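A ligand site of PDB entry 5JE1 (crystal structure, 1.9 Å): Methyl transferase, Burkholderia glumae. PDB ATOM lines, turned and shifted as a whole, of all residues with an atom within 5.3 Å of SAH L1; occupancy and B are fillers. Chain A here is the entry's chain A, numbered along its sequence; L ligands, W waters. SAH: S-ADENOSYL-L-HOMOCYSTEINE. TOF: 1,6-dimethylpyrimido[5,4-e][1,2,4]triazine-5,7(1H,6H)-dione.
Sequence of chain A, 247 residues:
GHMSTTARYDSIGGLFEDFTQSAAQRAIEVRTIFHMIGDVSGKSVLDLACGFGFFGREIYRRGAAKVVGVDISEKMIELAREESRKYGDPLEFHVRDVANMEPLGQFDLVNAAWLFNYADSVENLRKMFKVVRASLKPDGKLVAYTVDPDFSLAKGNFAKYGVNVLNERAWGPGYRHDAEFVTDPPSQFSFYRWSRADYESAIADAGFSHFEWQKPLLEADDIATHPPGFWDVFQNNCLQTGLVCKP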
ATOM      1  N   TYR A   9     -15.146 -17.501 -17.555  1.00  0.00           N
ATOM      2  CA  TYR A   9     -14.042 -17.925 -16.695  1.00  0.00           C
ATOM      3  C   TYR A   9     -14.423 -19.019 -15.721  1.00  0.00           C
ATOM      4  O   TYR A   9     -13.547 -19.516 -15.013  1.00  0.00           O
ATOM      5  CB  TYR A   9     -13.491 -16.735 -15.925  1.00  0.00           C
ATOM      6  CG  TYR A   9     -12.452 -15.986 -16.729  1.00  0.00           C
ATOM      7  CD1 TYR A   9     -11.114 -16.022 -16.367  1.00  0.00           C
ATOM      8  CD2 TYR A   9     -12.819 -15.272 -17.868  1.00  0.00           C
ATOM      9  CE1 TYR A   9     -10.165 -15.322 -17.117  1.00  0.00           C
ATOM     10  CE2 TYR A   9     -11.884 -14.587 -18.617  1.00  0.00           C
ATOM     11  CZ  TYR A   9     -10.560 -14.622 -18.235  1.00  0.00           C
ATOM     12  OH  TYR A   9      -9.646 -13.915 -18.974  1.00  0.00           O
ATOM     13  N   PHE A  16      -6.145 -19.400 -14.769  1.00  0.00           N
ATOM     14  CA  PHE A  16      -5.730 -18.017 -14.960  1.00  0.00           C
ATOM     15  C   PHE A  16      -4.542 -17.692 -14.067  1.00  0.00           C
ATOM     16  O   PHE A  16      -3.593 -17.023 -14.504  1.00  0.00           O
ATOM     17  CB  PHE A  16      -6.872 -17.043 -14.690  1.00  0.00           C
ATOM     18  CG  PHE A  16      -6.466 -15.611 -14.884  1.00  0.00           C
ATOM     19  CD1 PHE A  16      -6.141 -15.161 -16.169  1.00  0.00           C
ATOM     20  CD2 PHE A  16      -6.337 -14.755 -13.806  1.00  0.00           C
ATOM     21  CE1 PHE A  16      -5.738 -13.863 -16.355  1.00  0.00           C
ATOM     22  CE2 PHE A  16      -5.920 -13.442 -13.993  1.00  0.00           C
ATOM     23  CZ  PHE A  16      -5.624 -12.993 -15.268  1.00  0.00           C
ATOM     24  N   THR A  20      -0.773 -16.261 -14.956  1.00  0.00           N
ATOM     25  CA  THR A  20      -0.105 -15.074 -14.418  1.00  0.00           C
ATOM     26  C   THR A  20       1.287 -15.410 -13.889  1.00  0.00           C
ATOM     27  O   THR A  20       2.132 -14.507 -13.798  1.00  0.00           O
ATOM     28  CB  THR A  20      -0.926 -14.408 -13.293  1.00  0.00           C
ATOM     29  OG1 THR A  20      -0.950 -15.260 -12.139  1.00  0.00           O
ATOM     30  CG2 THR A  20      -2.344 -14.110 -13.740  1.00  0.00           C
ATOM     31  N   ARG A  26       2.951 -10.606 -18.046  1.00  0.00           N
ATOM     32  CA  ARG A  26       2.292 -10.288 -16.782  1.00  0.00           C
ATOM     33  C   ARG A  26       3.097  -9.279 -15.975  1.00  0.00           C
ATOM     34  O   ARG A  26       2.533  -8.320 -15.423  1.00  0.00           O
ATOM     35  CB  ARG A  26       2.040 -11.558 -15.970  1.00  0.00           C
ATOM     36  CG  ARG A  26       1.307 -11.330 -14.649  1.00  0.00           C
ATOM     37  CD  ARG A  26      -0.115 -10.750 -14.872  1.00  0.00           C
ATOM     38  NE  ARG A  26      -0.878 -10.748 -13.627  1.00  0.00           N
ATOM     39  CZ  ARG A  26      -2.161 -10.384 -13.508  1.00  0.00           C
ATOM     40  NH1 ARG A  26      -2.850  -9.995 -14.573  1.00  0.00           N
ATOM     41  NH2 ARG A  26      -2.761 -10.430 -12.324  1.00  0.00           N
ATOM     42  N   GLU A  29       2.391  -5.848 -17.255  1.00  0.00           N
ATOM     43  CA  GLU A  29       1.062  -5.388 -16.821  1.00  0.00           C
ATOM     44  C   GLU A  29       1.087  -4.890 -15.388  1.00  0.00           C
ATOM     45  O   GLU A  29       0.600  -3.788 -15.077  1.00  0.00           O
ATOM     46  CB  GLU A  29       0.040  -6.524 -16.915  1.00  0.00           C
ATOM     47  CG  GLU A  29      -0.075  -7.259 -18.221  1.00  0.00           C
ATOM     48  CD  GLU A  29      -0.912  -8.523 -18.081  1.00  0.00           C
ATOM     49  OE1 GLU A  29      -1.851  -8.551 -17.242  1.00  0.00           O
ATOM     50  OE2 GLU A  29      -0.613  -9.494 -18.808  1.00  0.00           O
ATOM     51  N   ASP A  47     -12.211  -2.921  -7.188  1.00  0.00           N
ATOM     52  CA  ASP A  47     -11.470  -3.696  -8.195  1.00  0.00           C
ATOM     53  C   ASP A  47     -12.490  -4.439  -9.065  1.00  0.00           C
ATOM     54  O   ASP A  47     -13.111  -5.402  -8.605  1.00  0.00           O
ATOM     55  CB  ASP A  47     -10.496  -4.630  -7.492  1.00  0.00           C
ATOM     56  CG  ASP A  47      -9.474  -5.292  -8.420  1.00  0.00           C
ATOM     57  OD1 ASP A  47      -9.079  -4.683  -9.456  1.00  0.00           O
ATOM     58  OD2 ASP A  47      -9.010  -6.405  -8.069  1.00  0.00           O
ATOM     59  N   LEU A  48     -12.667  -3.996 -10.311  1.00  0.00           N
ATOM     60  CA  LEU A  48     -13.643  -4.563 -11.223  1.00  0.00           C
ATOM     61  C   LEU A  48     -12.991  -5.604 -12.132  1.00  0.00           C
ATOM     62  O   LEU A  48     -11.835  -5.458 -12.530  1.00  0.00           O
ATOM     63  CB  LEU A  48     -14.278  -3.480 -12.090  1.00  0.00           C
ATOM     64  CG  LEU A  48     -14.975  -2.389 -11.274  1.00  0.00           C
ATOM     65  CD1 LEU A  48     -15.491  -1.283 -12.174  1.00  0.00           C
ATOM     66  CD2 LEU A  48     -16.102  -3.042 -10.474  1.00  0.00           C
ATOM     67  N   ALA A  49     -13.758  -6.655 -12.476  1.00  0.00           N
ATOM     68  CA  ALA A  49     -13.204  -7.833 -13.145  1.00  0.00           C
ATOM     69  C   ALA A  49     -12.006  -8.379 -12.350  1.00  0.00           C
ATOM     70  O   ALA A  49     -10.914  -8.554 -12.878  1.00  0.00           O
ATOM     71  CB  ALA A  49     -12.808  -7.519 -14.593  1.00  0.00           C
ATOM     72  N   CYS A  50     -12.230  -8.648 -11.057  1.00  0.00           N
ATOM     73  CA  CYS A  50     -11.125  -8.848 -10.121  1.00  0.00           C
ATOM     74  C   CYS A  50     -10.477 -10.223 -10.228  1.00  0.00           C
ATOM     75  O   CYS A  50      -9.366 -10.391  -9.695  1.00  0.00           O
ATOM     76  CB  CYS A  50     -11.594  -8.627  -8.684  1.00  0.00           C
ATOM     77  SG  CYS A  50     -12.901  -9.762  -8.143  1.00  0.00           S
ATOM     78  N   GLY A  51     -11.104 -11.184 -10.911  1.00  0.00           N
ATOM     79  CA  GLY A  51     -10.514 -12.519 -11.009  1.00  0.00           C
ATOM     80  C   GLY A  51     -10.393 -13.133  -9.621  1.00  0.00           C
ATOM     81  O   GLY A  51     -11.316 -13.027  -8.801  1.00  0.00           O
ATOM     82  N   PHE A  52      -9.245 -13.738  -9.322  1.00  0.00           N
ATOM     83  CA  PHE A  52      -9.050 -14.217  -7.964  1.00  0.00           C
ATOM     84  C   PHE A  52      -8.663 -13.105  -6.996  1.00  0.00           C
ATOM     85  O   PHE A  52      -8.393 -13.380  -5.821  1.00  0.00           O
ATOM     86  CB  PHE A  52      -8.018 -15.365  -7.910  1.00  0.00           C
ATOM     87  CG  PHE A  52      -6.658 -15.008  -8.445  1.00  0.00           C
ATOM     88  CD1 PHE A  52      -5.667 -14.515  -7.599  1.00  0.00           C
ATOM     89  CD2 PHE A  52      -6.351 -15.208  -9.791  1.00  0.00           C
ATOM     90  CE1 PHE A  52      -4.404 -14.201  -8.080  1.00  0.00           C
ATOM     91  CE2 PHE A  52      -5.088 -14.893 -10.281  1.00  0.00           C
ATOM     92  CZ  PHE A  52      -4.119 -14.379  -9.426  1.00  0.00           C
ATOM     93  N   PHE A  54      -6.181 -10.499  -7.485  1.00  0.00           N
ATOM     94  CA  PHE A  54      -4.776 -10.110  -7.401  1.00  0.00           C
ATOM     95  C   PHE A  54      -4.589  -8.625  -7.084  1.00  0.00           C
ATOM     96  O   PHE A  54      -3.903  -8.248  -6.126  1.00  0.00           O
ATOM     97  CB  PHE A  54      -4.054 -10.436  -8.715  1.00  0.00           C
ATOM     98  CG  PHE A  54      -2.610  -9.994  -8.695  1.00  0.00           C
ATOM     99  CD1 PHE A  54      -1.655 -10.777  -8.072  1.00  0.00           C
ATOM    100  CD2 PHE A  54      -2.239  -8.760  -9.237  1.00  0.00           C
ATOM    101  CE1 PHE A  54      -0.322 -10.364  -8.018  1.00  0.00           C
ATOM    102  CE2 PHE A  54      -0.927  -8.341  -9.184  1.00  0.00           C
ATOM    103  CZ  PHE A  54       0.041  -9.139  -8.580  1.00  0.00           C
ATOM    104  N   PHE A  55      -5.153  -7.758  -7.919  1.00  0.00           N
ATOM    105  CA  PHE A  55      -4.825  -6.350  -7.789  1.00  0.00           C
ATOM    106  C   PHE A  55      -5.421  -5.760  -6.513  1.00  0.00           C
ATOM    107  O   PHE A  55      -4.728  -5.063  -5.765  1.00  0.00           O
ATOM    108  CB  PHE A  55      -5.266  -5.589  -9.041  1.00  0.00           C
ATOM    109  CG  PHE A  55      -4.339  -5.821 -10.194  1.00  0.00           C
ATOM    110  CD1 PHE A  55      -3.076  -5.238 -10.210  1.00  0.00           C
ATOM    111  CD2 PHE A  55      -4.671  -6.688 -11.228  1.00  0.00           C
ATOM    112  CE1 PHE A  55      -2.196  -5.472 -11.252  1.00  0.00           C
ATOM    113  CE2 PHE A  55      -3.798  -6.929 -12.270  1.00  0.00           C
ATOM    114  CZ  PHE A  55      -2.550  -6.318 -12.287  1.00  0.00           C
ATOM    115  N   VAL A  70     -15.313  -7.133  -7.623  1.00  0.00           N
ATOM    116  CA  VAL A  70     -16.496  -7.520  -8.382  1.00  0.00           C
ATOM    117  C   VAL A  70     -16.070  -8.318  -9.602  1.00  0.00           C
ATOM    118  O   VAL A  70     -15.125  -7.927 -10.303  1.00  0.00           O
ATOM    119  CB  VAL A  70     -17.305  -6.281  -8.815  1.00  0.00           C
ATOM    120  CG1 VAL A  70     -18.455  -6.698  -9.723  1.00  0.00           C
ATOM    121  CG2 VAL A  70     -17.809  -5.507  -7.591  1.00  0.00           C
ATOM    122  N   ASP A  71     -16.741  -9.438  -9.854  1.00  0.00           N
ATOM    123  CA  ASP A  71     -16.469 -10.266 -11.020  1.00  0.00           C
ATOM    124  C   ASP A  71     -17.764 -10.947 -11.429  1.00  0.00           C
ATOM    125  O   ASP A  71     -18.588 -11.275 -10.574  1.00  0.00           O
ATOM    126  CB  ASP A  71     -15.378 -11.314 -10.744  1.00  0.00           C
ATOM    127  CG  ASP A  71     -14.713 -11.845 -12.025  1.00  0.00           C
ATOM    128  OD1 ASP A  71     -15.302 -12.693 -12.735  1.00  0.00           O
ATOM    129  OD2 ASP A  71     -13.570 -11.415 -12.300  1.00  0.00           O
ATOM    130  N   ILE A  72     -17.930 -11.166 -12.736  1.00  0.00           N
ATOM    131  CA  ILE A  72     -19.108 -11.843 -13.257  1.00  0.00           C
ATOM    132  C   ILE A  72     -19.079 -13.350 -12.985  1.00  0.00           C
ATOM    133  O   ILE A  72     -20.135 -13.991 -12.979  1.00  0.00           O
ATOM    134  CB  ILE A  72     -19.242 -11.555 -14.755  1.00  0.00           C
ATOM    135  CG1 ILE A  72     -20.635 -11.921 -15.281  1.00  0.00           C
ATOM    136  CG2 ILE A  72     -18.180 -12.315 -15.567  1.00  0.00           C
ATOM    137  CD1 ILE A  72     -20.865 -11.455 -16.719  1.00  0.00           C
ATOM    138  N   SER A  73     -17.890 -13.930 -12.758  1.00  0.00           N
ATOM    139  CA  SER A  73     -17.739 -15.386 -12.662  1.00  0.00           C
ATOM    140  C   SER A  73     -17.861 -15.863 -11.218  1.00  0.00           C
ATOM    141  O   SER A  73     -17.036 -15.517 -10.371  1.00  0.00           O
ATOM    142  CB  SER A  73     -16.378 -15.804 -13.230  1.00  0.00           C
ATOM    143  OG  SER A  73     -16.148 -17.167 -12.920  1.00  0.00           O
ATOM    144  N   MET A  76     -14.616 -17.569 -10.265  1.00  0.00           N
ATOM    145  CA  MET A  76     -13.497 -16.697  -9.905  1.00  0.00           C
ATOM    146  C   MET A  76     -13.740 -16.049  -8.548  1.00  0.00           C
ATOM    147  O   MET A  76     -12.804 -15.866  -7.763  1.00  0.00           O
ATOM    148  CB  MET A  76     -13.272 -15.643 -10.985  1.00  0.00           C
ATOM    149  CG  MET A  76     -13.017 -16.236 -12.366  1.00  0.00           C
ATOM    150  SD  MET A  76     -11.511 -17.240 -12.519  1.00  0.00           S
ATOM    151  CE  MET A  76     -10.241 -16.009 -12.264  1.00  0.00           C
ATOM    152  N   ARG A  96     -21.164  -9.770 -10.033  1.00  0.00           N
ATOM    153  CA  ARG A  96     -21.956  -8.806 -10.790  1.00  0.00           C
ATOM    154  C   ARG A  96     -21.459  -8.763 -12.224  1.00  0.00           C
ATOM    155  O   ARG A  96     -20.276  -8.991 -12.490  1.00  0.00           O
ATOM    156  CB  ARG A  96     -21.839  -7.398 -10.197  1.00  0.00           C
ATOM    157  CG  ARG A  96     -22.192  -7.272  -8.746  1.00  0.00           C
ATOM    158  CD  ARG A  96     -23.684  -7.173  -8.577  1.00  0.00           C
ATOM    159  NE  ARG A  96     -24.013  -6.733  -7.226  1.00  0.00           N
ATOM    160  CZ  ARG A  96     -24.126  -7.553  -6.193  1.00  0.00           C
ATOM    161  NH1 ARG A  96     -23.927  -8.854  -6.357  1.00  0.00           N
ATOM    162  NH2 ARG A  96     -24.430  -7.065  -4.995  1.00  0.00           N
ATOM    163  N   ASP A  97     -22.376  -8.465 -13.149  1.00  0.00           N
ATOM    164  CA  ASP A  97     -21.996  -8.045 -14.493  1.00  0.00           C
ATOM    165  C   ASP A  97     -21.850  -6.530 -14.468  1.00  0.00           C
ATOM    166  O   ASP A  97     -22.814  -5.820 -14.185  1.00  0.00           O
ATOM    167  CB  ASP A  97     -23.034  -8.495 -15.531  1.00  0.00           C
ATOM    168  CG  ASP A  97     -22.691  -8.046 -16.967  1.00  0.00           C
ATOM    169  OD1 ASP A  97     -21.654  -7.391 -17.214  1.00  0.00           O
ATOM    170  OD2 ASP A  97     -23.483  -8.359 -17.867  1.00  0.00           O
ATOM    171  N   VAL A  98     -20.631  -6.034 -14.748  1.00  0.00           N
ATOM    172  CA  VAL A  98     -20.380  -4.617 -14.538  1.00  0.00           C
ATOM    173  C   VAL A  98     -21.208  -3.758 -15.489  1.00  0.00           C
ATOM    174  O   VAL A  98     -21.624  -2.650 -15.128  1.00  0.00           O
ATOM    175  CB  VAL A  98     -18.870  -4.301 -14.642  1.00  0.00           C
ATOM    176  CG1 VAL A  98     -18.639  -2.799 -14.657  1.00  0.00           C
ATOM    177  CG2 VAL A  98     -18.144  -4.907 -13.444  1.00  0.00           C
ATOM    178  N   ALA A  99     -21.518  -4.271 -16.675  1.00  0.00           N
ATOM    179  CA  ALA A  99     -22.350  -3.517 -17.599  1.00  0.00           C
ATOM    180  C   ALA A  99     -23.781  -3.368 -17.104  1.00  0.00           C
ATOM    181  O   ALA A  99     -24.516  -2.522 -17.625  1.00  0.00           O
ATOM    182  CB  ALA A  99     -22.346  -4.201 -18.960  1.00  0.00           C
ATOM    183  N   ALA A 113      -8.584  -3.845 -14.364  1.00  0.00           N
ATOM    184  CA  ALA A 113      -7.602  -4.531 -15.200  1.00  0.00           C
ATOM    185  C   ALA A 113      -8.311  -5.654 -15.952  1.00  0.00           C
ATOM    186  O   ALA A 113      -8.780  -6.624 -15.344  1.00  0.00           O
ATOM    187  CB  ALA A 113      -6.459  -5.075 -14.344  1.00  0.00           C
ATOM    188  N   TRP A 114      -8.381  -5.524 -17.281  1.00  0.00           N
ATOM    189  CA  TRP A 114      -8.996  -6.524 -18.152  1.00  0.00           C
ATOM    190  C   TRP A 114     -10.503  -6.643 -17.930  1.00  0.00           C
ATOM    191  O   TRP A 114     -11.063  -7.747 -17.854  1.00  0.00           O
ATOM    192  CB  TRP A 114      -8.316  -7.884 -18.020  1.00  0.00           C
ATOM    193  CG  TRP A 114      -6.845  -7.806 -18.299  1.00  0.00           C
ATOM    194  CD1 TRP A 114      -5.833  -7.991 -17.413  1.00  0.00           C
ATOM    195  CD2 TRP A 114      -6.226  -7.495 -19.561  1.00  0.00           C
ATOM    196  NE1 TRP A 114      -4.625  -7.828 -18.033  1.00  0.00           N
ATOM    197  CE2 TRP A 114      -4.835  -7.524 -19.351  1.00  0.00           C
ATOM    198  CE3 TRP A 114      -6.711  -7.204 -20.843  1.00  0.00           C
ATOM    199  CZ2 TRP A 114      -3.919  -7.281 -20.382  1.00  0.00           C
ATOM    200  CZ3 TRP A 114      -5.796  -6.947 -21.865  1.00  0.00           C
ATOM    201  CH2 TRP A 114      -4.424  -6.996 -21.624  1.00  0.00           C
ATOM    202  N   LEU A 115     -11.172  -5.495 -17.829  1.00  0.00           N
ATOM    203  CA  LEU A 115     -12.624  -5.418 -17.800  1.00  0.00           C
ATOM    204  C   LEU A 115     -13.219  -5.029 -19.157  1.00  0.00           C
ATOM    205  O   LEU A 115     -14.092  -5.718 -19.672  1.00  0.00           O
ATOM    206  CB  LEU A 115     -13.074  -4.404 -16.753  1.00  0.00           C
ATOM    207  CG  LEU A 115     -14.559  -4.045 -16.851  1.00  0.00           C
ATOM    208  CD1 LEU A 115     -15.379  -5.269 -16.513  1.00  0.00           C
ATOM    209  CD2 LEU A 115     -14.918  -2.840 -15.956  1.00  0.00           C
ATOM    210  N   TYR A 118     -13.966  -7.046 -22.359  1.00  0.00           N
ATOM    211  CA  TYR A 118     -15.018  -8.046 -22.311  1.00  0.00           C
ATOM    212  C   TYR A 118     -16.412  -7.449 -22.495  1.00  0.00           C
ATOM    213  O   TYR A 118     -17.401  -8.194 -22.474  1.00  0.00           O
ATOM    214  CB  TYR A 118     -14.928  -8.843 -20.991  1.00  0.00           C
ATOM    215  CG  TYR A 118     -13.663  -9.700 -20.930  1.00  0.00           C
ATOM    216  CD1 TYR A 118     -13.510 -10.815 -21.746  1.00  0.00           C
ATOM    217  CD2 TYR A 118     -12.625  -9.375 -20.074  1.00  0.00           C
ATOM    218  CE1 TYR A 118     -12.354 -11.598 -21.697  1.00  0.00           C
ATOM    219  CE2 TYR A 118     -11.454 -10.143 -20.016  1.00  0.00           C
ATOM    220  CZ  TYR A 118     -11.316 -11.244 -20.823  1.00  0.00           C
ATOM    221  OH  TYR A 118     -10.160 -11.997 -20.746  1.00  0.00           O
ATOM    222  N   MET A 128     -20.502   0.361 -19.007  1.00  0.00           N
ATOM    223  CA  MET A 128     -19.466   0.120 -18.007  1.00  0.00           C
ATOM    224  C   MET A 128     -18.831   1.429 -17.546  1.00  0.00           C
ATOM    225  O   MET A 128     -18.668   1.656 -16.340  1.00  0.00           O
ATOM    226  CB  MET A 128     -18.393  -0.823 -18.568  1.00  0.00           C
ATOM    227  CG  MET A 128     -18.864  -2.254 -18.784  1.00  0.00           C
ATOM    228  SD  MET A 128     -17.443  -3.236 -19.338  1.00  0.00           S
ATOM    229  CE  MET A 128     -18.163  -4.874 -19.568  1.00  0.00           C
HETATM  230  N   SAH L   1      -8.165  -8.279 -13.009  1.00  0.00           N
HETATM  231  CA  SAH L   1      -7.653  -9.622 -12.745  1.00  0.00           C
HETATM  232  CB  SAH L   1      -8.420 -10.720 -13.517  1.00  0.00           C
HETATM  233  CG  SAH L   1      -8.546 -10.466 -15.004  1.00  0.00           C
HETATM  234  SD  SAH L   1      -9.239 -11.910 -15.786  1.00  0.00           S
HETATM  235  C   SAH L   1      -6.160  -9.751 -12.951  1.00  0.00           C
HETATM  236  O   SAH L   1      -5.529 -10.475 -12.126  1.00  0.00           O
HETATM  237  OXT SAH L   1      -5.579  -9.175 -13.918  1.00  0.00           O
HETATM  238  C5' SAH L   1     -10.653 -11.184 -16.539  1.00  0.00           C
HETATM  239  C4' SAH L   1     -11.814 -11.295 -15.552  1.00  0.00           C
HETATM  240  O4' SAH L   1     -12.893 -10.444 -15.927  1.00  0.00           O
HETATM  241  C3' SAH L   1     -12.406 -12.694 -15.407  1.00  0.00           C
HETATM  242  O3' SAH L   1     -12.384 -13.063 -14.012  1.00  0.00           O
HETATM  243  C2' SAH L   1     -13.848 -12.555 -15.883  1.00  0.00           C
HETATM  244  O2' SAH L   1     -14.773 -13.406 -15.185  1.00  0.00           O
HETATM  245  C1' SAH L   1     -14.120 -11.092 -15.587  1.00  0.00           C
HETATM  246  N9  SAH L   1     -15.200 -10.494 -16.388  1.00  0.00           N
HETATM  247  C8  SAH L   1     -15.410 -10.658 -17.717  1.00  0.00           C
HETATM  248  N7  SAH L   1     -16.493  -9.929 -18.105  1.00  0.00           N
HETATM  249  C5  SAH L   1     -16.945  -9.282 -17.014  1.00  0.00           C
HETATM  250  C6  SAH L   1     -18.057  -8.363 -16.732  1.00  0.00           C
HETATM  251  N6  SAH L   1     -18.886  -8.004 -17.742  1.00  0.00           N
HETATM  252  N1  SAH L   1     -18.210  -7.916 -15.464  1.00  0.00           N
HETATM  253  C2  SAH L   1     -17.382  -8.290 -14.463  1.00  0.00           C
HETATM  254  N3  SAH L   1     -16.348  -9.142 -14.658  1.00  0.00           N
HETATM  255  C4  SAH L   1     -16.093  -9.655 -15.893  1.00  0.00           C
HETATM  256  C1  TOF L   2      -5.019 -10.202 -22.652  1.00  0.00           C
HETATM  257  O1  TOF L   2      -3.997  -9.990 -23.292  1.00  0.00           O
HETATM  258  C2  TOF L   2      -5.004 -10.548 -21.218  1.00  0.00           C
HETATM  259  O2  TOF L   2      -8.420 -10.292 -23.092  1.00  0.00           O
HETATM  260  N3  TOF L   2      -3.899 -10.655 -20.518  1.00  0.00           N
HETATM  261  C4  TOF L   2      -3.958 -10.969 -19.225  1.00  0.00           C
HETATM  262  N5  TOF L   2      -5.101 -11.181 -18.623  1.00  0.00           N
HETATM  263  N6  TOF L   2      -6.219 -11.097 -19.251  1.00  0.00           N
HETATM  264  C7  TOF L   2      -6.245 -10.787 -20.562  1.00  0.00           C
HETATM  265  N8  TOF L   2      -7.384 -10.685 -21.221  1.00  0.00           N
HETATM  266  C9  TOF L   2      -7.367 -10.373 -22.513  1.00  0.00           C
HETATM  267  N10 TOF L   2      -6.248 -10.134 -23.227  1.00  0.00           N
HETATM  268  C11 TOF L   2      -7.480 -11.343 -18.565  1.00  0.00           C
HETATM  269  C12 TOF L   2      -6.347  -9.804 -24.648  1.00  0.00           C
HETATM  270  O   HOH W   1     -19.129  -8.634 -20.546  1.00  0.00           O
HETATM  271  O   HOH W   2      -7.536  -8.164  -9.679  1.00  0.00           O
HETATM  272  O   HOH W   3     -16.130 -14.711 -17.318  1.00  0.00           O
HETATM  273  O   HOH W   4      -9.153  -5.619 -11.993  1.00  0.00           O
HETATM  274  O   HOH W   5     -17.447 -11.679 -20.197  1.00  0.00           O
HETATM  275  O   HOH W   6     -15.075 -13.251 -19.979  1.00  0.00           O
HETATM  276  O   HOH W   7      -6.765 -11.951 -10.112  1.00  0.00           O
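Water W7 lies within hydrogen-bond range of O of SAH L1 (2.8 Å), N of Phe 54 (3.1 Å), O of Cys 50 (3.1 Å) and N of Phe 52 (3.2 Å). Water W3 bridges an oxygen (O2') of SAH L1 (2.8 Å) and the backbone NH (N) of Tyr 9 (3.0 Å). Water W1 lies within hydrogen-bond range of the backbone carbonyl oxygen (O) of Tyr 118 (2.6 Å) and a nitrogen (N6) of SAH L1 (2.9 Å). Water W4 lies within hydrogen-bond range of the side-chain carboxylate of Asp 47 (2.7 Å), the backbone carbonyl oxygen of Leu 48 (2.7 Å), a nitrogen (N) of SAH L1 (3.0 Å) and the backbone NH of Ala 113 (3.0 Å). Water W2 lies within hydrogen-bond range of the side-chain carboxylate (OD2) of Asp 47 (2.8 Å), the backbone carbonyl oxygen (O) of Cys 50 (2.9 Å), the backbone NH (N) of Phe 55 (3.0 Å), a nitrogen (N) of SAH L1 (3.4 Å) and the backbone NH (N) of Phe 54 (3.5 Å).
Residues that only touch SAH L1: Phe 16, Cys 50, Gly 51, Phe 54, Phe 55, Ser 73, Met 76, Arg 96, Trp 114, Tyr 118 and Met 128. Of the 27 residues printed, 19 come within 4 Å of SAH L1. Along chain A the residues within 4 Å of SAH L1 span positions 9 to 128.
An oxygen (O2') of SAH L1 lies within hydrogen-bond range of the side-chain carboxylate (OD1) of Asp 71, at 2.6 Å. The backbone carbonyl oxygen (O) of Ala 49 is in hydrogen-bond range of a nitrogen (N) of SAH L1, 2.8 Å away. The guanidinium group (NH2) of Arg 26 is in salt-bridge range of an oxygen (O) of SAH L1 (2.8 Å). The side-chain carboxylate (OD1) of Asp 97 sits at hydrogen-bond distance from a nitrogen (N6) of SAH L1 (2.9 Å). O of Ala 113 lies within hydrogen-bond range of N of SAH L1 (2.9 Å). The backbone NH of Val 98 lies within hydrogen-bond range of a nitrogen (N1) of SAH L1, 3.1 Å away. The backbone NH (N) of Ile 72 sits at hydrogen-bond distance from a nitrogen (N3) of SAH L1, 3.2 Å away. OH of Tyr 9 lies close to SD of SAH L1 (3.8 Å). The side-chain hydroxyl (OH) of Tyr 118 lies within hydrogen-bond range of a nitrogen (N8) of TOF L2, 3.1 Å away. A nitrogen (N5) of TOF L2 lies close to the indole nitrogen (NE1) of Trp 114 (3.4 Å).
N of Ser 73 lies within hydrogen-bond range of OD1 of Asp 71 (2.9 Å). The backbone carbonyl oxygen of Asp 71 is in hydrogen-bond range of the backbone NH of Arg 96, 3.0 Å away. N of Cys 50 lies within hydrogen-bond range of OD2 of Asp 71, at 3.3 Å. The backbone carbonyl oxygen (O) of Val 70 is in hydrogen-bond range of the backbone NH (N) of Ala 49. OD1 of Asp 97 is in hydrogen-bond range of N of Ala 99, 3.2 Å away. OH of Tyr 9 is in hydrogen-bond range of OH of Tyr 118 (2.7 Å). The side-chain hydroxyl of Ser 73 sits at hydrogen-bond distance from the backbone NH of Met 76 (3.1 Å). N of Cys 50 sits at hydrogen-bond distance from O of Val 70 (3.1 Å).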
